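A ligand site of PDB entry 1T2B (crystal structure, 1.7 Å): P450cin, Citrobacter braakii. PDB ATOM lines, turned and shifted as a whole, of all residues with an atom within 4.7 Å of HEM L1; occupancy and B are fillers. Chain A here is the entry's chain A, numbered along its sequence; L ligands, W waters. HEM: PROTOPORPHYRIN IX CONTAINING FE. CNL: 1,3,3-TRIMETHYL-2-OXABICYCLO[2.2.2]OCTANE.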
ATOM      1  N   ILE A  58     -21.840 -26.809 -28.893  1.00  0.00           N
ATOM      2  CA  ILE A  58     -23.118 -26.991 -28.218  1.00  0.00           C
ATOM      3  C   ILE A  58     -24.323 -26.952 -29.173  1.00  0.00           C
ATOM      4  O   ILE A  58     -25.385 -27.486 -28.867  1.00  0.00           O
ATOM      5  CB  ILE A  58     -23.242 -25.925 -27.049  1.00  0.00           C
ATOM      6  CG1 ILE A  58     -24.143 -26.470 -25.937  1.00  0.00           C
ATOM      7  CG2 ILE A  58     -23.739 -24.600 -27.593  1.00  0.00           C
ATOM      8  CD1 ILE A  58     -24.080 -25.619 -24.627  1.00  0.00           C
ATOM      9  N   ASN A  66     -25.058 -35.737 -25.389  1.00  0.00           N
ATOM     10  CA  ASN A  66     -25.109 -35.392 -23.985  1.00  0.00           C
ATOM     11  C   ASN A  66     -24.891 -36.579 -23.044  1.00  0.00           C
ATOM     12  O   ASN A  66     -24.981 -36.436 -21.822  1.00  0.00           O
ATOM     13  CB  ASN A  66     -26.390 -34.622 -23.651  1.00  0.00           C
ATOM     14  CG  ASN A  66     -26.170 -33.137 -23.707  1.00  0.00           C
ATOM     15  OD1 ASN A  66     -25.731 -32.601 -24.730  1.00  0.00           O
ATOM     16  ND2 ASN A  66     -26.444 -32.452 -22.602  1.00  0.00           N
ATOM     17  N   VAL A  69     -22.477 -35.513 -20.656  1.00  0.00           N
ATOM     18  CA  VAL A  69     -22.772 -34.294 -19.893  1.00  0.00           C
ATOM     19  C   VAL A  69     -21.925 -34.125 -18.610  1.00  0.00           C
ATOM     20  O   VAL A  69     -21.476 -33.010 -18.312  1.00  0.00           O
ATOM     21  CB  VAL A  69     -24.294 -34.156 -19.585  1.00  0.00           C
ATOM     22  CG1 VAL A  69     -24.778 -35.266 -18.661  1.00  0.00           C
ATOM     23  CG2 VAL A  69     -24.585 -32.757 -19.020  1.00  0.00           C
ATOM     24  N   MET A  83     -33.116 -35.769 -19.126  1.00  0.00           N
ATOM     25  CA  MET A  83     -32.995 -34.592 -19.964  1.00  0.00           C
ATOM     26  C   MET A  83     -31.528 -34.222 -20.232  1.00  0.00           C
ATOM     27  O   MET A  83     -31.069 -34.294 -21.376  1.00  0.00           O
ATOM     28  CB  MET A  83     -33.731 -33.392 -19.341  1.00  0.00           C
ATOM     29  CG  MET A  83     -35.258 -33.565 -19.206  1.00  0.00           C
ATOM     30  SD  MET A  83     -36.043 -32.187 -18.306  1.00  0.00           S
ATOM     31  CE  MET A  83     -35.611 -32.686 -16.623  1.00  0.00           C
ATOM     32  N   ALA A  84     -30.793 -33.864 -19.184  1.00  0.00           N
ATOM     33  CA  ALA A  84     -29.395 -33.457 -19.352  1.00  0.00           C
ATOM     34  C   ALA A  84     -28.477 -34.552 -19.917  1.00  0.00           C
ATOM     35  O   ALA A  84     -27.520 -34.243 -20.603  1.00  0.00           O
ATOM     36  CB  ALA A  84     -28.837 -32.954 -18.039  1.00  0.00           C
ATOM     37  N   HIS A  91     -34.738 -36.801 -25.237  1.00  0.00           N
ATOM     38  CA  HIS A  91     -34.619 -35.583 -24.444  1.00  0.00           C
ATOM     39  C   HIS A  91     -35.797 -34.622 -24.541  1.00  0.00           C
ATOM     40  O   HIS A  91     -36.317 -34.163 -23.536  1.00  0.00           O
ATOM     41  CB  HIS A  91     -33.313 -34.866 -24.827  1.00  0.00           C
ATOM     42  CG  HIS A  91     -33.322 -33.389 -24.551  1.00  0.00           C
ATOM     43  ND1 HIS A  91     -33.667 -32.461 -25.507  1.00  0.00           N
ATOM     44  CD2 HIS A  91     -33.047 -32.689 -23.424  1.00  0.00           C
ATOM     45  CE1 HIS A  91     -33.598 -31.248 -24.979  1.00  0.00           C
ATOM     46  NE2 HIS A  91     -33.226 -31.361 -23.720  1.00  0.00           N
ATOM     47  N   ARG A  95     -38.366 -33.525 -21.490  1.00  0.00           N
ATOM     48  CA  ARG A  95     -38.384 -32.137 -21.028  1.00  0.00           C
ATOM     49  C   ARG A  95     -39.765 -31.502 -21.182  1.00  0.00           C
ATOM     50  O   ARG A  95     -40.168 -30.677 -20.352  1.00  0.00           O
ATOM     51  CB  ARG A  95     -37.366 -31.292 -21.782  1.00  0.00           C
ATOM     52  CG  ARG A  95     -37.427 -29.834 -21.365  1.00  0.00           C
ATOM     53  CD  ARG A  95     -36.152 -29.090 -21.644  1.00  0.00           C
ATOM     54  NE  ARG A  95     -36.299 -27.667 -21.338  1.00  0.00           N
ATOM     55  CZ  ARG A  95     -35.277 -26.812 -21.273  1.00  0.00           C
ATOM     56  NH1 ARG A  95     -34.044 -27.257 -21.471  1.00  0.00           N
ATOM     57  NH2 ARG A  95     -35.481 -25.531 -21.004  1.00  0.00           N
ATOM     58  N   PHE A 102     -41.695 -24.915 -14.909  1.00  0.00           N
ATOM     59  CA  PHE A 102     -40.523 -24.063 -14.954  1.00  0.00           C
ATOM     60  C   PHE A 102     -40.633 -22.836 -15.850  1.00  0.00           C
ATOM     61  O   PHE A 102     -39.647 -22.132 -16.053  1.00  0.00           O
ATOM     62  CB  PHE A 102     -39.306 -24.884 -15.367  1.00  0.00           C
ATOM     63  CG  PHE A 102     -38.798 -25.777 -14.280  1.00  0.00           C
ATOM     64  CD1 PHE A 102     -37.985 -25.273 -13.275  1.00  0.00           C
ATOM     65  CD2 PHE A 102     -39.150 -27.123 -14.242  1.00  0.00           C
ATOM     66  CE1 PHE A 102     -37.526 -26.114 -12.246  1.00  0.00           C
ATOM     67  CE2 PHE A 102     -38.693 -27.964 -13.227  1.00  0.00           C
ATOM     68  CZ  PHE A 102     -37.879 -27.459 -12.222  1.00  0.00           C
ATOM     69  N   LEU A 149     -40.158 -28.198  -4.250  1.00  0.00           N
ATOM     70  CA  LEU A 149     -40.400 -28.566  -5.649  1.00  0.00           C
ATOM     71  C   LEU A 149     -40.621 -30.072  -5.777  1.00  0.00           C
ATOM     72  O   LEU A 149     -41.455 -30.514  -6.558  1.00  0.00           O
ATOM     73  CB  LEU A 149     -39.200 -28.191  -6.527  1.00  0.00           C
ATOM     74  CG  LEU A 149     -38.909 -26.723  -6.877  1.00  0.00           C
ATOM     75  CD1 LEU A 149     -37.582 -26.603  -7.609  1.00  0.00           C
ATOM     76  CD2 LEU A 149     -40.035 -26.172  -7.737  1.00  0.00           C
ATOM     77  N   ILE A 227     -31.876 -35.139 -11.107  1.00  0.00           N
ATOM     78  CA  ILE A 227     -31.385 -33.935 -11.746  1.00  0.00           C
ATOM     79  C   ILE A 227     -31.962 -32.656 -11.156  1.00  0.00           C
ATOM     80  O   ILE A 227     -31.262 -31.655 -11.038  1.00  0.00           O
ATOM     81  CB  ILE A 227     -31.609 -33.954 -13.300  1.00  0.00           C
ATOM     82  CG1 ILE A 227     -30.776 -32.830 -13.952  1.00  0.00           C
ATOM     83  CG2 ILE A 227     -33.100 -33.831 -13.623  1.00  0.00           C
ATOM     84  CD1 ILE A 227     -30.882 -32.752 -15.470  1.00  0.00           C
ATOM     85  N   LEU A 228     -33.219 -32.688 -10.731  1.00  0.00           N
ATOM     86  CA  LEU A 228     -33.815 -31.499 -10.146  1.00  0.00           C
ATOM     87  C   LEU A 228     -33.179 -31.235  -8.780  1.00  0.00           C
ATOM     88  O   LEU A 228     -32.915 -30.097  -8.411  1.00  0.00           O
ATOM     89  CB  LEU A 228     -35.333 -31.646 -10.033  1.00  0.00           C
ATOM     90  CG  LEU A 228     -36.057 -31.817 -11.381  1.00  0.00           C
ATOM     91  CD1 LEU A 228     -37.539 -32.011 -11.109  1.00  0.00           C
ATOM     92  CD2 LEU A 228     -35.868 -30.603 -12.262  1.00  0.00           C
ATOM     93  N   GLY A 231     -29.707 -29.542  -9.452  1.00  0.00           N
ATOM     94  CA  GLY A 231     -29.815 -28.144  -9.834  1.00  0.00           C
ATOM     95  C   GLY A 231     -29.919 -27.183  -8.661  1.00  0.00           C
ATOM     96  O   GLY A 231     -29.242 -26.148  -8.633  1.00  0.00           O
ATOM     97  N   GLY A 232     -30.743 -27.518  -7.663  1.00  0.00           N
ATOM     98  CA  GLY A 232     -30.891 -26.642  -6.507  1.00  0.00           C
ATOM     99  C   GLY A 232     -29.779 -26.722  -5.470  1.00  0.00           C
ATOM    100  O   GLY A 232     -29.078 -25.729  -5.182  1.00  0.00           O
ATOM    101  N   ASN A 235     -25.740 -26.654  -8.001  1.00  0.00           N
ATOM    102  CA  ASN A 235     -25.572 -25.482  -8.838  1.00  0.00           C
ATOM    103  C   ASN A 235     -25.942 -24.157  -8.172  1.00  0.00           C
ATOM    104  O   ASN A 235     -25.100 -23.262  -8.021  1.00  0.00           O
ATOM    105  CB  ASN A 235     -26.376 -25.650 -10.112  1.00  0.00           C
ATOM    106  CG  ASN A 235     -26.011 -26.910 -10.876  1.00  0.00           C
ATOM    107  OD1 ASN A 235     -25.693 -27.934 -10.302  1.00  0.00           O
ATOM    108  ND2 ASN A 235     -26.065 -26.823 -12.186  1.00  0.00           N
ATOM    109  N   THR A 236     -27.207 -24.015  -7.780  1.00  0.00           N
ATOM    110  CA  THR A 236     -27.681 -22.773  -7.174  1.00  0.00           C
ATOM    111  C   THR A 236     -26.955 -22.378  -5.889  1.00  0.00           C
ATOM    112  O   THR A 236     -26.634 -21.210  -5.682  1.00  0.00           O
ATOM    113  CB  THR A 236     -29.188 -22.841  -6.883  1.00  0.00           C
ATOM    114  OG1 THR A 236     -29.880 -23.243  -8.087  1.00  0.00           O
ATOM    115  CG2 THR A 236     -29.703 -21.462  -6.449  1.00  0.00           C
ATOM    116  N   PHE A 239     -23.448 -21.013  -6.724  1.00  0.00           N
ATOM    117  CA  PHE A 239     -23.553 -19.692  -7.349  1.00  0.00           C
ATOM    118  C   PHE A 239     -23.847 -18.586  -6.295  1.00  0.00           C
ATOM    119  O   PHE A 239     -23.105 -17.606  -6.175  1.00  0.00           O
ATOM    120  CB  PHE A 239     -24.641 -19.690  -8.446  1.00  0.00           C
ATOM    121  CG  PHE A 239     -24.960 -18.320  -8.975  1.00  0.00           C
ATOM    122  CD1 PHE A 239     -26.234 -17.776  -8.792  1.00  0.00           C
ATOM    123  CD2 PHE A 239     -23.985 -17.551  -9.617  1.00  0.00           C
ATOM    124  CE1 PHE A 239     -26.532 -16.493  -9.253  1.00  0.00           C
ATOM    125  CE2 PHE A 239     -24.271 -16.271 -10.072  1.00  0.00           C
ATOM    126  CZ  PHE A 239     -25.552 -15.737  -9.896  1.00  0.00           C
ATOM    127  N   LEU A 272     -24.248 -13.995 -13.004  1.00  0.00           N
ATOM    128  CA  LEU A 272     -24.292 -15.341 -13.586  1.00  0.00           C
ATOM    129  C   LEU A 272     -23.133 -15.476 -14.592  1.00  0.00           C
ATOM    130  O   LEU A 272     -22.442 -16.474 -14.631  1.00  0.00           O
ATOM    131  CB  LEU A 272     -25.634 -15.595 -14.285  1.00  0.00           C
ATOM    132  CG  LEU A 272     -26.729 -16.108 -13.342  1.00  0.00           C
ATOM    133  CD1 LEU A 272     -28.089 -15.983 -14.029  1.00  0.00           C
ATOM    134  CD2 LEU A 272     -26.414 -17.581 -12.913  1.00  0.00           C
ATOM    135  N   PRO A 277     -21.404 -21.406 -12.135  1.00  0.00           N
ATOM    136  CA  PRO A 277     -20.699 -22.535 -11.458  1.00  0.00           C
ATOM    137  C   PRO A 277     -20.188 -23.579 -12.380  1.00  0.00           C
ATOM    138  O   PRO A 277     -19.103 -24.153 -12.242  1.00  0.00           O
ATOM    139  CB  PRO A 277     -21.751 -23.070 -10.499  1.00  0.00           C
ATOM    140  CG  PRO A 277     -22.753 -21.969 -10.365  1.00  0.00           C
ATOM    141  CD  PRO A 277     -22.877 -21.367 -11.742  1.00  0.00           C
ATOM    142  N   ALA A 278     -21.037 -23.788 -13.343  1.00  0.00           N
ATOM    143  CA  ALA A 278     -20.950 -24.899 -14.238  1.00  0.00           C
ATOM    144  C   ALA A 278     -19.948 -24.914 -15.359  1.00  0.00           C
ATOM    145  O   ALA A 278     -19.399 -23.917 -15.815  1.00  0.00           O
ATOM    146  CB  ALA A 278     -22.334 -25.123 -14.825  1.00  0.00           C
ATOM    147  N   VAL A 280     -19.872 -28.269 -18.677  1.00  0.00           N
ATOM    148  CA  VAL A 280     -20.551 -29.490 -19.084  1.00  0.00           C
ATOM    149  C   VAL A 280     -19.669 -30.210 -20.097  1.00  0.00           C
ATOM    150  O   VAL A 280     -18.808 -29.592 -20.741  1.00  0.00           O
ATOM    151  CB  VAL A 280     -21.941 -29.226 -19.752  1.00  0.00           C
ATOM    152  CG1 VAL A 280     -22.924 -28.605 -18.742  1.00  0.00           C
ATOM    153  CG2 VAL A 280     -21.762 -28.309 -20.983  1.00  0.00           C
ATOM    154  N   ARG A 282     -19.323 -33.179 -23.422  1.00  0.00           N
ATOM    155  CA  ARG A 282     -20.013 -33.718 -24.598  1.00  0.00           C
ATOM    156  C   ARG A 282     -19.185 -34.896 -25.096  1.00  0.00           C
ATOM    157  O   ARG A 282     -17.947 -34.816 -25.148  1.00  0.00           O
ATOM    158  CB  ARG A 282     -20.091 -32.700 -25.748  1.00  0.00           C
ATOM    159  CG  ARG A 282     -21.024 -31.508 -25.544  1.00  0.00           C
ATOM    160  CD  ARG A 282     -22.463 -31.959 -25.415  1.00  0.00           C
ATOM    161  NE  ARG A 282     -23.408 -30.839 -25.380  1.00  0.00           N
ATOM    162  CZ  ARG A 282     -23.856 -30.259 -24.277  1.00  0.00           C
ATOM    163  NH1 ARG A 282     -23.432 -30.659 -23.077  1.00  0.00           N
ATOM    164  NH2 ARG A 282     -24.755 -29.289 -24.356  1.00  0.00           N
ATOM    165  N   PHE A 305     -17.376 -23.009 -19.861  1.00  0.00           N
ATOM    166  CA  PHE A 305     -18.169 -21.786 -19.937  1.00  0.00           C
ATOM    167  C   PHE A 305     -17.537 -20.560 -19.261  1.00  0.00           C
ATOM    168  O   PHE A 305     -17.593 -19.475 -19.801  1.00  0.00           O
ATOM    169  CB  PHE A 305     -19.572 -22.004 -19.354  1.00  0.00           C
ATOM    170  CG  PHE A 305     -20.400 -23.023 -20.083  1.00  0.00           C
ATOM    171  CD1 PHE A 305     -21.169 -23.936 -19.360  1.00  0.00           C
ATOM    172  CD2 PHE A 305     -20.505 -23.020 -21.466  1.00  0.00           C
ATOM    173  CE1 PHE A 305     -22.027 -24.820 -19.985  1.00  0.00           C
ATOM    174  CE2 PHE A 305     -21.384 -23.911 -22.104  1.00  0.00           C
ATOM    175  CZ  PHE A 305     -22.137 -24.804 -21.367  1.00  0.00           C
ATOM    176  N   LEU A 331     -22.855 -17.851 -21.293  1.00  0.00           N
ATOM    177  CA  LEU A 331     -23.181 -19.273 -21.479  1.00  0.00           C
ATOM    178  C   LEU A 331     -23.329 -20.024 -20.158  1.00  0.00           C
ATOM    179  O   LEU A 331     -23.371 -21.256 -20.134  1.00  0.00           O
ATOM    180  CB  LEU A 331     -22.089 -19.959 -22.325  1.00  0.00           C
ATOM    181  CG  LEU A 331     -21.876 -19.369 -23.719  1.00  0.00           C
ATOM    182  CD1 LEU A 331     -20.691 -19.997 -24.404  1.00  0.00           C
ATOM    183  CD2 LEU A 331     -23.128 -19.583 -24.542  1.00  0.00           C
ATOM    184  N   SER A 332     -23.415 -19.295 -19.060  1.00  0.00           N
ATOM    185  CA  SER A 332     -23.533 -19.904 -17.748  1.00  0.00           C
ATOM    186  C   SER A 332     -24.737 -20.822 -17.543  1.00  0.00           C
ATOM    187  O   SER A 332     -24.727 -21.663 -16.660  1.00  0.00           O
ATOM    188  CB  SER A 332     -23.510 -18.829 -16.674  1.00  0.00           C
ATOM    189  OG  SER A 332     -22.259 -18.175 -16.716  1.00  0.00           O
ATOM    190  N   LEU A 333     -25.781 -20.629 -18.351  1.00  0.00           N
ATOM    191  CA  LEU A 333     -26.955 -21.485 -18.235  1.00  0.00           C
ATOM    192  C   LEU A 333     -27.084 -22.342 -19.486  1.00  0.00           C
ATOM    193  O   LEU A 333     -28.154 -22.870 -19.785  1.00  0.00           O
ATOM    194  CB  LEU A 333     -28.204 -20.637 -18.017  1.00  0.00           C
ATOM    195  CG  LEU A 333     -28.255 -19.924 -16.667  1.00  0.00           C
ATOM    196  CD1 LEU A 333     -29.460 -19.012 -16.604  1.00  0.00           C
ATOM    197  CD2 LEU A 333     -28.304 -20.959 -15.559  1.00  0.00           C
ATOM    198  N   GLY A 334     -25.982 -22.499 -20.215  1.00  0.00           N
ATOM    199  CA  GLY A 334     -26.032 -23.297 -21.418  1.00  0.00           C
ATOM    200  C   GLY A 334     -26.579 -22.527 -22.608  1.00  0.00           C
ATOM    201  O   GLY A 334     -26.769 -21.313 -22.548  1.00  0.00           O
ATOM    202  N   ILE A 337     -30.700 -26.644 -27.170  1.00  0.00           N
ATOM    203  CA  ILE A 337     -31.719 -27.560 -26.665  1.00  0.00           C
ATOM    204  C   ILE A 337     -31.605 -27.973 -25.201  1.00  0.00           C
ATOM    205  O   ILE A 337     -32.619 -28.317 -24.565  1.00  0.00           O
ATOM    206  CB  ILE A 337     -31.793 -28.839 -27.557  1.00  0.00           C
ATOM    207  CG1 ILE A 337     -30.539 -29.692 -27.376  1.00  0.00           C
ATOM    208  CG2 ILE A 337     -31.926 -28.410 -29.040  1.00  0.00           C
ATOM    209  CD1 ILE A 337     -30.620 -31.020 -28.117  1.00  0.00           C
ATOM    210  N   HIS A 338     -30.399 -27.908 -24.637  1.00  0.00           N
ATOM    211  CA  HIS A 338     -30.229 -28.289 -23.229  1.00  0.00           C
ATOM    212  C   HIS A 338     -30.140 -27.083 -22.269  1.00  0.00           C
ATOM    213  O   HIS A 338     -29.827 -27.261 -21.090  1.00  0.00           O
ATOM    214  CB  HIS A 338     -28.976 -29.148 -23.070  1.00  0.00           C
ATOM    215  CG  HIS A 338     -29.086 -30.502 -23.687  1.00  0.00           C
ATOM    216  ND1 HIS A 338     -29.826 -31.533 -23.124  1.00  0.00           N
ATOM    217  CD2 HIS A 338     -28.535 -31.019 -24.809  1.00  0.00           C
ATOM    218  CE1 HIS A 338     -29.715 -32.611 -23.878  1.00  0.00           C
ATOM    219  NE2 HIS A 338     -28.938 -32.331 -24.907  1.00  0.00           N
ATOM    220  N   ARG A 339     -30.444 -25.883 -22.779  1.00  0.00           N
ATOM    221  CA  ARG A 339     -30.362 -24.673 -21.961  1.00  0.00           C
ATOM    222  C   ARG A 339     -31.131 -24.866 -20.655  1.00  0.00           C
ATOM    223  O   ARG A 339     -32.264 -25.389 -20.647  1.00  0.00           O
ATOM    224  CB  ARG A 339     -30.909 -23.471 -22.706  1.00  0.00           C
ATOM    225  CG  ARG A 339     -30.290 -22.145 -22.270  1.00  0.00           C
ATOM    226  CD  ARG A 339     -31.340 -21.187 -21.819  1.00  0.00           C
ATOM    227  NE  ARG A 339     -30.825 -19.824 -21.698  1.00  0.00           N
ATOM    228  CZ  ARG A 339     -31.463 -18.845 -21.074  1.00  0.00           C
ATOM    229  NH1 ARG A 339     -32.642 -19.065 -20.517  1.00  0.00           N
ATOM    230  NH2 ARG A 339     -30.919 -17.634 -21.029  1.00  0.00           N
ATOM    231  N   CYS A 340     -30.505 -24.462 -19.550  1.00  0.00           N
ATOM    232  CA  CYS A 340     -31.064 -24.652 -18.197  1.00  0.00           C
ATOM    233  C   CYS A 340     -32.587 -24.559 -18.054  1.00  0.00           C
ATOM    234  O   CYS A 340     -33.178 -23.514 -18.304  1.00  0.00           O
ATOM    235  CB  CYS A 340     -30.431 -23.669 -17.210  1.00  0.00           C
ATOM    236  SG  CYS A 340     -30.852 -24.099 -15.477  1.00  0.00           S
ATOM    237  N   LEU A 341     -33.194 -25.660 -17.614  1.00  0.00           N
ATOM    238  CA  LEU A 341     -34.641 -25.732 -17.373  1.00  0.00           C
ATOM    239  C   LEU A 341     -34.994 -24.776 -16.228  1.00  0.00           C
ATOM    240  O   LEU A 341     -36.097 -24.212 -16.172  1.00  0.00           O
ATOM    241  CB  LEU A 341     -35.013 -27.167 -16.963  1.00  0.00           C
ATOM    242  CG  LEU A 341     -36.402 -27.785 -17.161  1.00  0.00           C
ATOM    243  CD1 LEU A 341     -36.758 -28.545 -15.894  1.00  0.00           C
ATOM    244  CD2 LEU A 341     -37.440 -26.770 -17.544  1.00  0.00           C
ATOM    245  N   GLY A 342     -34.051 -24.597 -15.298  1.00  0.00           N
ATOM    246  CA  GLY A 342     -34.306 -23.731 -14.172  1.00  0.00           C
ATOM    247  C   GLY A 342     -33.893 -22.278 -14.344  1.00  0.00           C
ATOM    248  O   GLY A 342     -33.812 -21.540 -13.365  1.00  0.00           O
ATOM    249  N   LEU A 345     -36.315 -19.621 -12.857  1.00  0.00           N
ATOM    250  CA  LEU A 345     -36.390 -19.834 -11.412  1.00  0.00           C
ATOM    251  C   LEU A 345     -35.154 -19.302 -10.684  1.00  0.00           C
ATOM    252  O   LEU A 345     -35.260 -18.600  -9.662  1.00  0.00           O
ATOM    253  CB  LEU A 345     -36.549 -21.323 -11.120  1.00  0.00           C
ATOM    254  CG  LEU A 345     -36.684 -21.698  -9.626  1.00  0.00           C
ATOM    255  CD1 LEU A 345     -37.992 -21.149  -9.063  1.00  0.00           C
ATOM    256  CD2 LEU A 345     -36.635 -23.206  -9.473  1.00  0.00           C
ATOM    257  N   ILE A 346     -33.970 -19.629 -11.189  1.00  0.00           N
ATOM    258  CA  ILE A 346     -32.798 -19.160 -10.475  1.00  0.00           C
ATOM    259  C   ILE A 346     -32.644 -17.642 -10.617  1.00  0.00           C
ATOM    260  O   ILE A 346     -32.086 -17.018  -9.723  1.00  0.00           O
ATOM    261  CB  ILE A 346     -31.552 -19.952 -10.905  1.00  0.00           C
ATOM    262  CG1 ILE A 346     -30.974 -19.402 -12.179  1.00  0.00           C
ATOM    263  CG2 ILE A 346     -31.899 -21.433 -11.004  1.00  0.00           C
ATOM    264  CD1 ILE A 346     -29.733 -18.602 -11.905  1.00  0.00           C
HETATM  265  CHA HEM L   1     -29.163 -27.686 -17.682  1.00  0.00           C
HETATM  266  CHB HEM L   1     -26.517 -24.387 -15.318  1.00  0.00           C
HETATM  267  CHC HEM L   1     -29.797 -24.433 -11.652  1.00  0.00           C
HETATM  268  CHD HEM L   1     -32.337 -27.960 -13.966  1.00  0.00           C
HETATM  269  C1A HEM L   1     -28.199 -26.704 -17.403  1.00  0.00           C
HETATM  270  C2A HEM L   1     -27.061 -26.391 -18.282  1.00  0.00           C
HETATM  271  C3A HEM L   1     -26.304 -25.498 -17.566  1.00  0.00           C
HETATM  272  C4A HEM L   1     -26.977 -25.281 -16.275  1.00  0.00           C
HETATM  273  CMA HEM L   1     -24.946 -24.960 -17.928  1.00  0.00           C
HETATM  274  CAA HEM L   1     -26.781 -26.866 -19.735  1.00  0.00           C
HETATM  275  CBA HEM L   1     -26.522 -28.364 -19.798  1.00  0.00           C
HETATM  276  CGA HEM L   1     -25.829 -28.824 -21.087  1.00  0.00           C
HETATM  277  O1A HEM L   1     -25.589 -27.992 -21.984  1.00  0.00           O
HETATM  278  O2A HEM L   1     -25.547 -30.038 -21.193  1.00  0.00           O
HETATM  279  C1B HEM L   1     -27.180 -24.155 -14.078  1.00  0.00           C
HETATM  280  C2B HEM L   1     -26.761 -23.132 -13.137  1.00  0.00           C
HETATM  281  C3B HEM L   1     -27.694 -23.154 -12.102  1.00  0.00           C
HETATM  282  C4B HEM L   1     -28.644 -24.181 -12.419  1.00  0.00           C
HETATM  283  CMB HEM L   1     -25.562 -22.199 -13.234  1.00  0.00           C
HETATM  284  CAB HEM L   1     -27.895 -22.289 -10.975  1.00  0.00           C
HETATM  285  CBB HEM L   1     -27.384 -21.055 -10.769  1.00  0.00           C
HETATM  286  C1C HEM L   1     -30.814 -25.356 -11.995  1.00  0.00           C
HETATM  287  C2C HEM L   1     -32.006 -25.640 -11.210  1.00  0.00           C
HETATM  288  C3C HEM L   1     -32.717 -26.602 -11.853  1.00  0.00           C
HETATM  289  C4C HEM L   1     -31.920 -26.960 -13.017  1.00  0.00           C
HETATM  290  CMC HEM L   1     -32.373 -24.898  -9.972  1.00  0.00           C
HETATM  291  CAC HEM L   1     -33.997 -27.109 -11.650  1.00  0.00           C
HETATM  292  CBC HEM L   1     -34.603 -27.279 -10.448  1.00  0.00           C
HETATM  293  C1D HEM L   1     -31.670 -28.204 -15.206  1.00  0.00           C
HETATM  294  C2D HEM L   1     -32.063 -29.203 -16.136  1.00  0.00           C
HETATM  295  C3D HEM L   1     -31.179 -29.140 -17.165  1.00  0.00           C
HETATM  296  C4D HEM L   1     -30.230 -28.083 -16.848  1.00  0.00           C
HETATM  297  CMD HEM L   1     -33.237 -30.200 -15.935  1.00  0.00           C
HETATM  298  CAD HEM L   1     -31.142 -30.025 -18.380  1.00  0.00           C
HETATM  299  CBD HEM L   1     -32.015 -29.344 -19.418  1.00  0.00           C
HETATM  300  CGD HEM L   1     -32.065 -30.097 -20.742  1.00  0.00           C
HETATM  301  O1D HEM L   1     -32.853 -29.695 -21.622  1.00  0.00           O
HETATM  302  O2D HEM L   1     -31.309 -31.072 -20.896  1.00  0.00           O
HETATM  303  NA  HEM L   1     -28.174 -25.977 -16.197  1.00  0.00           N
HETATM  304  NB  HEM L   1     -28.366 -24.758 -13.673  1.00  0.00           N
HETATM  305  NC  HEM L   1     -30.800 -26.139 -13.156  1.00  0.00           N
HETATM  306  ND  HEM L   1     -30.542 -27.493 -15.654  1.00  0.00           N
HETATM  307 FE   HEM L   1     -29.636 -25.883 -14.765  1.00  0.00          FE
HETATM  308  C1  CNL L   2     -26.959 -30.329 -13.739  1.00  0.00           C
HETATM  309  C2  CNL L   2     -27.572 -30.482 -15.185  1.00  0.00           C
HETATM  310  C3  CNL L   2     -26.422 -30.723 -16.262  1.00  0.00           C
HETATM  311  C4  CNL L   2     -24.974 -30.708 -15.556  1.00  0.00           C
HETATM  312  C5  CNL L   2     -25.010 -31.909 -14.514  1.00  0.00           C
HETATM  313  C6  CNL L   2     -26.175 -31.682 -13.429  1.00  0.00           C
HETATM  314  C7  CNL L   2     -28.055 -30.072 -12.705  1.00  0.00           C
HETATM  315  C8  CNL L   2     -24.825 -29.319 -14.758  1.00  0.00           C
HETATM  316  C9  CNL L   2     -24.832 -28.088 -15.687  1.00  0.00           C
HETATM  317  C10 CNL L   2     -23.509 -29.146 -13.992  1.00  0.00           C
HETATM  318  O   CNL L   2     -25.957 -29.209 -13.791  1.00  0.00           O
HETATM  319  O   HOH W   1     -27.137 -26.100 -23.155  1.00  0.00           O
HETATM  320  O   HOH W   2     -22.548 -21.723 -14.916  1.00  0.00           O
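The backbone carbonyl oxygen (O) of Met 83 sits close to an oxygen (O2D) of HEM L1 (3.3 Å).
ND2 of Asn 235 lies close to NB of HEM L1, 3.4 Å away.
The backbone carbonyl oxygen of Ile 337 sits close to an oxygen (O1D) of HEM L1, 3.3 Å away.
Ile 58 touches HEM L1.
CG2 of Val 69 touches O2A of HEM L1 (3.6 Å).
Phe 102 touches HEM L1.
Ile 227 touches HEM L1.
Leu 228 touches HEM L1.
Gly 231 touches HEM L1 (O to CHC, 3.5 Å).
Gly 232 touches HEM L1 (N to CMC, 3.9 Å).
Thr 236 touches HEM L1.
Phe 239 touches HEM L1 (CB to CBB, 3.8 Å).
CD of Pro 277 touches CMB of HEM L1, at 3.2 Å.
Val 280 touches HEM L1.
CE1 of Phe 305 touches CMA of HEM L1 (3.6 Å).
Ser 332 touches HEM L1 (O to CHB, 3.5 Å).
Leu 333 touches HEM L1.
Gly 334 touches HEM L1.
Leu 341 touches HEM L1 (CB to CMD, 3.7 Å).
N of Gly 342 touches C4C of HEM L1, 3.9 Å away.
CD1 of Ile 346 touches CBB of HEM L1, 3.6 Å away.
Hydrophobic or aromatic side chains within 4 Å of HEM L1: Ile 58, Val 69, Met 83, Ala 84, His 91, Phe 102, Ile 227, Leu 228, Phe 239, Pro 277, Val 280, Phe 305, Leu 333, His 338, Leu 341 and Ile 346.
SG of Cys 340 is bound to FE of HEM L1.
The backbone NH (N) of Ala 84 sits at hydrogen-bond distance from an oxygen (O2D) of HEM L1, at 3.3 Å.
NH1 of Arg 95 lies within salt-bridge range of O1D of HEM L1.
The side-chain amide nitrogen of Asn 66 sits at hydrogen-bond distance from an oxygen (O2A) of HEM L1 (2.9 Å).
A ring nitrogen (NE2) of His 91 is in hydrogen-bond range of an oxygen (O1D) of HEM L1.
NH2 of Arg 282 lies within salt-bridge range of O1A of HEM L1, at 2.8 Å.
An oxygen (O) of CNL L2 lies within hydrogen-bond range of the side-chain amide nitrogen of Asn 235.
ND1 of His 338 lies within hydrogen-bond range of O2D of HEM L1, 2.7 Å away.
NE2 of His 91 lies close to ND1 of His 338 (3.5 Å).
A ring nitrogen (NE2) of His 91 lies close to the backbone carbonyl oxygen (O) of Ile 337 (3.2 Å).
The backbone NH of Gly 342 lies close to the side-chain sulfur of Cys 340, 3.2 Å away.
A ring nitrogen (ND1) of His 338 sits close to the backbone carbonyl oxygen (O) of Met 83 (3.5 Å).
The side-chain amide oxygen (OD1) of Asn 66 sits at hydrogen-bond distance from the guanidinium group (NE) of Arg 282 (3.0 Å).
The side-chain hydroxyl (OG) of Ser 332 is in hydrogen-bond range of the backbone carbonyl oxygen (O) of Leu 272, 2.7 Å away.
The backbone carbonyl oxygen (O) of Gly 231 lies within hydrogen-bond range of the side-chain hydroxyl (OG1) of Thr 236, 3.0 Å away.
A ring nitrogen (NE2) of His 338 sits close to the side-chain amide oxygen of Asn 66, 3.2 Å away.
Water W1 lies within hydrogen-bond range of O1A of HEM L1 and N of Arg 339.
Water W2 lies within hydrogen-bond range of the backbone carbonyl oxygen of Ser 332 and the backbone NH of Ala 278.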
